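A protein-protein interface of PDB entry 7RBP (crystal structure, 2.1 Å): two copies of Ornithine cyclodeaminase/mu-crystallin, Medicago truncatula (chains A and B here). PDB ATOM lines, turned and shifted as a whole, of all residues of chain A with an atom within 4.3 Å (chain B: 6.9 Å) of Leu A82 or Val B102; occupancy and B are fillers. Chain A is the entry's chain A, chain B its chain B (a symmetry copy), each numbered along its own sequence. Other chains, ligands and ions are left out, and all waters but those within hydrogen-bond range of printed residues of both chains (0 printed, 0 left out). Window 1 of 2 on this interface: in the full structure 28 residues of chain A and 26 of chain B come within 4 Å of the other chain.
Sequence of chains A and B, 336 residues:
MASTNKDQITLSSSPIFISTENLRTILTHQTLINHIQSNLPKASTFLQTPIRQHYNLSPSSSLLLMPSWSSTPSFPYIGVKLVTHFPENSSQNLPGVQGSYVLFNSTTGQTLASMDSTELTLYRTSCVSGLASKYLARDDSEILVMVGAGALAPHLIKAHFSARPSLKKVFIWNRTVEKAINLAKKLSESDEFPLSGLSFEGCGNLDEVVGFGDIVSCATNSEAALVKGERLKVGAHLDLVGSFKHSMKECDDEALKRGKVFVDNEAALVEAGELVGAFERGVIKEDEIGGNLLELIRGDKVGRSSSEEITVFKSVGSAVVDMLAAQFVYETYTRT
O of Ser A100 lies within hydrogen-bond range of N of Leu A82 (2.9 Å). The backbone carbonyl oxygen (O) of Val B80 is in hydrogen-bond range of the backbone NH (N) of Val B102 (2.9 Å). The backbone carbonyl oxygen of Gly A99 is in hydrogen-bond range of the backbone NH of Ser A117 (3.1 Å). The backbone NH (N) of Phe B104 lies within hydrogen-bond range of the backbone carbonyl oxygen (O) of Ile B78 (2.8 Å).
Among the printed residues, merely in contact across the chains: Leu A65 with Leu B65, Leu A82 with Val B102, Leu A82 with Phe B104 and Gly A99 with Thr B111.
Leu A82 touches just these residues of chain B: Val B102 (3.9 Å) and Phe B104 (3.8 Å). Of the printed residues of chain A, Phe B104 touches Leu A82 (3.8 Å). Of the printed residues of chain A, Thr B111 touches Gly A99 (3.5 Å). Printed residues of chain A within 4 Å of Leu B65: Leu A65 (3.99 Å). Leu B103 touches none of the printed residues of chain A. The nearest printed residue of chain B that does not touch Leu A82 is Val B80 (4.2 Å).
Of the 19 printed residues of chain B, 4 touch a printed residue of chain A. Among the printed residues, 4 pairs touch across the chains.
Leu A65 touches its own counterpart, Leu B65. Positions printed for both chains: 65, 80, 81, 82 and 100. Of the 4 pairs that touch across the chains among the printed residues, 1 has its exchanged pair printed and touching as well.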
ATOM      1  N   LEU A  64      -8.778 -10.728   2.187  1.00  0.00           N
ATOM      2  CA  LEU A  64      -8.428 -12.038   2.715  1.00  0.00           C
ATOM      3  C   LEU A  64      -8.359 -11.967   4.234  1.00  0.00           C
ATOM      4  O   LEU A  64      -7.795 -11.022   4.795  1.00  0.00           O
ATOM      5  CB  LEU A  64      -7.072 -12.527   2.178  1.00  0.00           C
ATOM      6  CG  LEU A  64      -6.863 -12.937   0.715  1.00  0.00           C
ATOM      7  CD1 LEU A  64      -7.786 -14.084   0.338  1.00  0.00           C
ATOM      8  CD2 LEU A  64      -7.012 -11.767  -0.256  1.00  0.00           C
ATOM      9  N   LEU A  65      -8.927 -12.974   4.893  1.00  0.00           N
ATOM     10  CA  LEU A  65      -8.800 -13.151   6.333  1.00  0.00           C
ATOM     11  C   LEU A  65      -8.187 -14.516   6.603  1.00  0.00           C
ATOM     12  O   LEU A  65      -8.697 -15.535   6.122  1.00  0.00           O
ATOM     13  CB  LEU A  65     -10.154 -13.031   7.042  1.00  0.00           C
ATOM     14  CG  LEU A  65     -11.112 -11.911   6.630  1.00  0.00           C
ATOM     15  CD1 LEU A  65     -12.402 -12.004   7.436  1.00  0.00           C
ATOM     16  CD2 LEU A  65     -10.470 -10.544   6.800  1.00  0.00           C
ATOM     17  N   VAL A  80      -5.103 -13.226  13.550  1.00  0.00           N
ATOM     18  CA  VAL A  80      -5.858 -13.015  12.323  1.00  0.00           C
ATOM     19  C   VAL A  80      -5.097 -12.009  11.474  1.00  0.00           C
ATOM     20  O   VAL A  80      -4.864 -10.874  11.906  1.00  0.00           O
ATOM     21  CB  VAL A  80      -7.293 -12.528  12.585  1.00  0.00           C
ATOM     22  CG1 VAL A  80      -8.140 -12.711  11.334  1.00  0.00           C
ATOM     23  CG2 VAL A  80      -7.915 -13.274  13.754  1.00  0.00           C
ATOM     24  N   LYS A  81      -4.696 -12.427  10.280  1.00  0.00           N
ATOM     25  CA  LYS A  81      -4.136 -11.523   9.287  1.00  0.00           C
ATOM     26  C   LYS A  81      -5.261 -11.074   8.361  1.00  0.00           C
ATOM     27  O   LYS A  81      -5.948 -11.911   7.768  1.00  0.00           O
ATOM     28  CB  LYS A  81      -3.018 -12.203   8.493  1.00  0.00           C
ATOM     29  CG  LYS A  81      -2.068 -11.245   7.777  1.00  0.00           C
ATOM     30  CD  LYS A  81      -0.863 -11.984   7.193  1.00  0.00           C
ATOM     31  CE  LYS A  81      -0.116 -11.125   6.183  1.00  0.00           C
ATOM     32  NZ  LYS A  81       0.976 -11.876   5.498  1.00  0.00           N
ATOM     33  N   LEU A  82      -5.473  -9.763   8.273  1.00  0.00           N
ATOM     34  CA  LEU A  82      -6.430  -9.172   7.345  1.00  0.00           C
ATOM     35  C   LEU A  82      -5.638  -8.459   6.261  1.00  0.00           C
ATOM     36  O   LEU A  82      -4.847  -7.561   6.563  1.00  0.00           O
ATOM     37  CB  LEU A  82      -7.363  -8.183   8.045  1.00  0.00           C
ATOM     38  CG  LEU A  82      -7.771  -8.360   9.507  1.00  0.00           C
ATOM     39  CD1 LEU A  82      -8.584  -7.158   9.959  1.00  0.00           C
ATOM     40  CD2 LEU A  82      -8.571  -9.628   9.698  1.00  0.00           C
ATOM     41  N   VAL A  83      -5.849  -8.853   5.006  1.00  0.00           N
ATOM     42  CA  VAL A  83      -5.069  -8.334   3.888  1.00  0.00           C
ATOM     43  C   VAL A  83      -6.013  -7.876   2.786  1.00  0.00           C
ATOM     44  O   VAL A  83      -6.919  -8.614   2.388  1.00  0.00           O
ATOM     45  CB  VAL A  83      -4.076  -9.384   3.349  1.00  0.00           C
ATOM     46  CG1 VAL A  83      -3.351  -8.851   2.123  1.00  0.00           C
ATOM     47  CG2 VAL A  83      -3.074  -9.777   4.425  1.00  0.00           C
ATOM     48  N   GLN A  98      -2.031  -4.420   1.382  1.00  0.00           N
ATOM     49  CA  GLN A  98      -2.045  -3.731   2.668  1.00  0.00           C
ATOM     50  C   GLN A  98      -2.790  -4.582   3.684  1.00  0.00           C
ATOM     51  O   GLN A  98      -3.392  -5.598   3.341  1.00  0.00           O
ATOM     52  CB  GLN A  98      -2.695  -2.343   2.554  1.00  0.00           C
ATOM     53  CG  GLN A  98      -1.939  -1.370   1.662  1.00  0.00           C
ATOM     54  CD  GLN A  98      -2.791  -0.195   1.220  1.00  0.00           C
ATOM     55  OE1 GLN A  98      -2.657   0.913   1.739  1.00  0.00           O
ATOM     56  NE2 GLN A  98      -3.676  -0.433   0.256  1.00  0.00           N
ATOM     57  N   GLY A  99      -2.747  -4.176   4.943  1.00  0.00           N
ATOM     58  CA  GLY A  99      -3.572  -4.811   5.952  1.00  0.00           C
ATOM     59  C   GLY A  99      -2.939  -4.755   7.329  1.00  0.00           C
ATOM     60  O   GLY A  99      -2.023  -3.981   7.590  1.00  0.00           O
ATOM     61  N   SER A 100      -3.449  -5.627   8.198  1.00  0.00           N
ATOM     62  CA  SER A 100      -3.111  -5.626   9.615  1.00  0.00           C
ATOM     63  C   SER A 100      -3.053  -7.051  10.142  1.00  0.00           C
ATOM     64  O   SER A 100      -3.796  -7.928   9.697  1.00  0.00           O
ATOM     65  CB  SER A 100      -4.138  -4.825  10.428  1.00  0.00           C
ATOM     66  OG  SER A 100      -3.680  -4.590  11.747  1.00  0.00           O
ATOM     67  N   SER A 117       0.562  -5.507   8.441  1.00  0.00           N
ATOM     68  CA  SER A 117       0.845  -6.831   7.901  1.00  0.00           C
ATOM     69  C   SER A 117       1.949  -6.797   6.850  1.00  0.00           C
ATOM     70  O   SER A 117       2.726  -7.749   6.743  1.00  0.00           O
ATOM     71  CB  SER A 117      -0.423  -7.434   7.297  1.00  0.00           C
ATOM     72  OG  SER A 117      -0.915  -6.611   6.254  1.00  0.00           O
ATOM     73  N   PRO B  15      -2.849   3.518  10.151  1.00  0.00           N
ATOM     74  CA  PRO B  15      -4.142   3.375  10.822  1.00  0.00           C
ATOM     75  C   PRO B  15      -4.083   3.959  12.224  1.00  0.00           C
ATOM     76  O   PRO B  15      -3.016   4.113  12.821  1.00  0.00           O
ATOM     77  CB  PRO B  15      -4.359   1.858  10.857  1.00  0.00           C
ATOM     78  CG  PRO B  15      -2.972   1.296  10.877  1.00  0.00           C
ATOM     79  CD  PRO B  15      -2.125   2.237  10.056  1.00  0.00           C
ATOM     80  N   LEU B  65     -15.484 -13.862  13.005  1.00  0.00           N
ATOM     81  CA  LEU B  65     -15.047 -12.861  12.045  1.00  0.00           C
ATOM     82  C   LEU B  65     -16.264 -12.372  11.272  1.00  0.00           C
ATOM     83  O   LEU B  65     -16.993 -13.179  10.686  1.00  0.00           O
ATOM     84  CB  LEU B  65     -14.006 -13.430  11.077  1.00  0.00           C
ATOM     85  CG  LEU B  65     -12.794 -14.171  11.651  1.00  0.00           C
ATOM     86  CD1 LEU B  65     -11.746 -14.380  10.568  1.00  0.00           C
ATOM     87  CD2 LEU B  65     -12.200 -13.433  12.835  1.00  0.00           C
ATOM     88  N   ILE B  78     -14.459  -0.691   4.180  1.00  0.00           N
ATOM     89  CA  ILE B  78     -14.464  -2.094   4.566  1.00  0.00           C
ATOM     90  C   ILE B  78     -14.362  -2.142   6.086  1.00  0.00           C
ATOM     91  O   ILE B  78     -13.621  -1.361   6.687  1.00  0.00           O
ATOM     92  CB  ILE B  78     -13.298  -2.867   3.919  1.00  0.00           C
ATOM     93  CG1 ILE B  78     -13.269  -2.644   2.405  1.00  0.00           C
ATOM     94  CG2 ILE B  78     -13.375  -4.353   4.248  1.00  0.00           C
ATOM     95  CD1 ILE B  78     -11.882  -2.782   1.804  1.00  0.00           C
ATOM     96  N   GLY B  79     -15.115  -3.034   6.706  1.00  0.00           N
ATOM     97  CA  GLY B  79     -15.038  -3.224   8.137  1.00  0.00           C
ATOM     98  C   GLY B  79     -14.925  -4.700   8.455  1.00  0.00           C
ATOM     99  O   GLY B  79     -15.467  -5.548   7.748  1.00  0.00           O
ATOM    100  N   VAL B  80     -14.177  -4.998   9.512  1.00  0.00           N
ATOM    101  CA  VAL B  80     -14.047  -6.373   9.989  1.00  0.00           C
ATOM    102  C   VAL B  80     -14.119  -6.352  11.510  1.00  0.00           C
ATOM    103  O   VAL B  80     -13.301  -5.701  12.164  1.00  0.00           O
ATOM    104  CB  VAL B  80     -12.742  -7.047   9.526  1.00  0.00           C
ATOM    105  CG1 VAL B  80     -12.731  -8.493   9.949  1.00  0.00           C
ATOM    106  CG2 VAL B  80     -12.578  -6.953   8.013  1.00  0.00           C
ATOM    107  N   LYS B  81     -15.100  -7.054  12.071  1.00  0.00           N
ATOM    108  CA  LYS B  81     -15.219  -7.225  13.512  1.00  0.00           C
ATOM    109  C   LYS B  81     -14.642  -8.581  13.896  1.00  0.00           C
ATOM    110  O   LYS B  81     -15.046  -9.608  13.339  1.00  0.00           O
ATOM    111  CB  LYS B  81     -16.681  -7.121  13.956  1.00  0.00           C
ATOM    112  CG  LYS B  81     -16.881  -6.722  15.413  1.00  0.00           C
ATOM    113  CD  LYS B  81     -18.306  -6.221  15.659  1.00  0.00           C
ATOM    114  CE  LYS B  81     -19.083  -7.149  16.579  1.00  0.00           C
ATOM    115  NZ  LYS B  81     -20.419  -6.596  16.949  1.00  0.00           N
ATOM    116  N   LEU B  82     -13.691  -8.582  14.826  1.00  0.00           N
ATOM    117  CA  LEU B  82     -13.095  -9.800  15.360  1.00  0.00           C
ATOM    118  C   LEU B  82     -13.504  -9.921  16.820  1.00  0.00           C
ATOM    119  O   LEU B  82     -13.211  -9.026  17.623  1.00  0.00           O
ATOM    120  CB  LEU B  82     -11.572  -9.776  15.229  1.00  0.00           C
ATOM    121  CG  LEU B  82     -11.001  -9.163  13.952  1.00  0.00           C
ATOM    122  CD1 LEU B  82      -9.486  -9.098  14.017  1.00  0.00           C
ATOM    123  CD2 LEU B  82     -11.431  -9.985  12.767  1.00  0.00           C
ATOM    124  N   SER B 100     -11.962  -6.513  18.527  1.00  0.00           N
ATOM    125  CA  SER B 100     -11.575  -5.270  17.872  1.00  0.00           C
ATOM    126  C   SER B 100     -12.311  -5.125  16.544  1.00  0.00           C
ATOM    127  O   SER B 100     -12.580  -6.108  15.851  1.00  0.00           O
ATOM    128  CB  SER B 100     -10.056  -5.204  17.627  1.00  0.00           C
ATOM    129  OG  SER B 100      -9.712  -4.178  16.706  1.00  0.00           O
ATOM    130  N   TYR B 101     -12.626  -3.882  16.192  1.00  0.00           N
ATOM    131  CA  TYR B 101     -13.211  -3.556  14.897  1.00  0.00           C
ATOM    132  C   TYR B 101     -12.182  -2.793  14.074  1.00  0.00           C
ATOM    133  O   TYR B 101     -11.649  -1.775  14.529  1.00  0.00           O
ATOM    134  CB  TYR B 101     -14.489  -2.728  15.056  1.00  0.00           C
ATOM    135  CG  TYR B 101     -15.316  -2.635  13.790  1.00  0.00           C
ATOM    136  CD1 TYR B 101     -16.508  -3.336  13.664  1.00  0.00           C
ATOM    137  CD2 TYR B 101     -14.903  -1.848  12.721  1.00  0.00           C
ATOM    138  CE1 TYR B 101     -17.265  -3.257  12.509  1.00  0.00           C
ATOM    139  CE2 TYR B 101     -15.651  -1.765  11.562  1.00  0.00           C
ATOM    140  CZ  TYR B 101     -16.830  -2.468  11.463  1.00  0.00           C
ATOM    141  OH  TYR B 101     -17.577  -2.383  10.312  1.00  0.00           O
ATOM    142  N   VAL B 102     -11.917  -3.278  12.863  1.00  0.00           N
ATOM    143  CA  VAL B 102     -10.878  -2.733  11.996  1.00  0.00           C
ATOM    144  C   VAL B 102     -11.546  -2.139  10.762  1.00  0.00           C
ATOM    145  O   VAL B 102     -12.316  -2.822  10.075  1.00  0.00           O
ATOM    146  CB  VAL B 102      -9.847  -3.802  11.602  1.00  0.00           C
ATOM    147  CG1 VAL B 102      -8.745  -3.191  10.757  1.00  0.00           C
ATOM    148  CG2 VAL B 102      -9.269  -4.461  12.845  1.00  0.00           C
ATOM    149  N   LEU B 103     -11.247  -0.873  10.483  1.00  0.00           N
ATOM    150  CA  LEU B 103     -11.805  -0.152   9.349  1.00  0.00           C
ATOM    151  C   LEU B 103     -10.731   0.032   8.283  1.00  0.00           C
ATOM    152  O   LEU B 103      -9.575   0.320   8.597  1.00  0.00           O
ATOM    153  CB  LEU B 103     -12.361   1.208   9.794  1.00  0.00           C
ATOM    154  CG  LEU B 103     -13.314   1.963   8.864  1.00  0.00           C
ATOM    155  CD1 LEU B 103     -14.669   1.270   8.793  1.00  0.00           C
ATOM    156  CD2 LEU B 103     -13.476   3.407   9.328  1.00  0.00           C
ATOM    157  N   PHE B 104     -11.120  -0.159   7.022  1.00  0.00           N
ATOM    158  CA  PHE B 104     -10.261   0.033   5.865  1.00  0.00           C
ATOM    159  C   PHE B 104     -10.943   0.976   4.884  1.00  0.00           C
ATOM    160  O   PHE B 104     -12.175   1.014   4.789  1.00  0.00           O
ATOM    161  CB  PHE B 104      -9.955  -1.280   5.113  1.00  0.00           C
ATOM    162  CG  PHE B 104      -9.326  -2.358   5.949  1.00  0.00           C
ATOM    163  CD1 PHE B 104     -10.096  -3.152   6.778  1.00  0.00           C
ATOM    164  CD2 PHE B 104      -7.965  -2.609   5.863  1.00  0.00           C
ATOM    165  CE1 PHE B 104      -9.518  -4.159   7.528  1.00  0.00           C
ATOM    166  CE2 PHE B 104      -7.382  -3.610   6.612  1.00  0.00           C
ATOM    167  CZ  PHE B 104      -8.156  -4.386   7.446  1.00  0.00           C
ATOM    168  N   THR B 111      -5.527   0.346   5.696  1.00  0.00           N
ATOM    169  CA  THR B 111      -6.065   0.281   7.047  1.00  0.00           C
ATOM    170  C   THR B 111      -6.186   1.693   7.607  1.00  0.00           C
ATOM    171  O   THR B 111      -5.202   2.438   7.652  1.00  0.00           O
ATOM    172  CB  THR B 111      -5.163  -0.574   7.940  1.00  0.00           C
ATOM    173  OG1 THR B 111      -4.761  -1.753   7.230  1.00  0.00           O
ATOM    174  CG2 THR B 111      -5.900  -0.976   9.211  1.00  0.00           C
ATOM    175  N   LEU B 112      -7.399   2.072   8.013  1.00  0.00           N
ATOM    176  CA  LEU B 112      -7.700   3.417   8.480  1.00  0.00           C
ATOM    177  C   LEU B 112      -7.734   3.524  10.000  1.00  0.00           C
ATOM    178  O   LEU B 112      -7.135   4.445  10.564  1.00  0.00           O
ATOM    179  CB  LEU B 112      -9.046   3.880   7.906  1.00  0.00           C
ATOM    180  CG  LEU B 112      -9.119   4.161   6.405  1.00  0.00           C
ATOM    181  CD1 LEU B 112     -10.524   4.608   6.031  1.00  0.00           C
ATOM    182  CD2 LEU B 112      -8.091   5.212   6.011  1.00  0.00           C
ATOM    183  N   ALA B 113      -8.430   2.611  10.674  1.00  0.00           N
ATOM    184  CA  ALA B 113      -8.599   2.716  12.115  1.00  0.00           C
ATOM    185  C   ALA B 113      -8.936   1.351  12.695  1.00  0.00           C
ATOM    186  O   ALA B 113      -9.424   0.457  11.997  1.00  0.00           O
ATOM    187  CB  ALA B 113      -9.689   3.732  12.477  1.00  0.00           C
ATOM    188  N   SER B 114      -8.663   1.212  13.990  1.00  0.00           N
ATOM    189  CA  SER B 114      -9.007   0.029  14.768  1.00  0.00           C
ATOM    190  C   SER B 114      -9.523   0.484  16.123  1.00  0.00           C
ATOM    191  O   SER B 114      -9.048   1.489  16.656  1.00  0.00           O
ATOM    192  CB  SER B 114      -7.802  -0.902  14.942  1.00  0.00           C
ATOM    193  OG  SER B 114      -7.005  -0.500  16.042  1.00  0.00           O
ATOM    194  N   MET B 115     -10.497  -0.242  16.667  1.00  0.00           N
ATOM    195  CA  MET B 115     -11.125   0.148  17.925  1.00  0.00           C
ATOM    196  C   MET B 115     -11.711  -1.084  18.600  1.00  0.00           C
ATOM    197  O   MET B 115     -11.935  -2.116  17.964  1.00  0.00           O
ATOM    198  CB  MET B 115     -12.209   1.205  17.703  1.00  0.00           C
ATOM    199  CG  MET B 115     -13.360   0.732  16.832  1.00  0.00           C
ATOM    200  SD  MET B 115     -14.290   2.080  16.079  1.00  0.00           S
ATOM    201  CE  MET B 115     -13.409   2.286  14.532  1.00  0.00           C
ATOM    202  N   MET B 323     -20.898  -0.932  11.155  1.00  0.00           N
ATOM    203  CA  MET B 323     -20.152  -0.135  10.187  1.00  0.00           C
ATOM    204  C   MET B 323     -20.504   1.341  10.302  1.00  0.00           C
ATOM    205  O   MET B 323     -19.618   2.200  10.237  1.00  0.00           O
ATOM    206  CB  MET B 323     -20.421  -0.635   8.769  1.00  0.00           C
ATOM    207  CG  MET B 323     -19.911   0.304   7.690  1.00  0.00           C
ATOM    208  SD  MET B 323     -18.123   0.536   7.763  1.00  0.00           S
ATOM    209  CE  MET B 323     -17.586  -0.873   6.800  1.00  0.00           C
ATOM    210  N   ALA B 326     -18.661   2.621  13.422  1.00  0.00           N
ATOM    211  CA  ALA B 326     -17.219   2.716  13.208  1.00  0.00           C
ATOM    212  C   ALA B 326     -16.881   3.871  12.275  1.00  0.00           C
ATOM    213  O   ALA B 326     -15.919   4.617  12.515  1.00  0.00           O
ATOM    214  CB  ALA B 326     -16.682   1.398  12.654  1.00  0.00           C
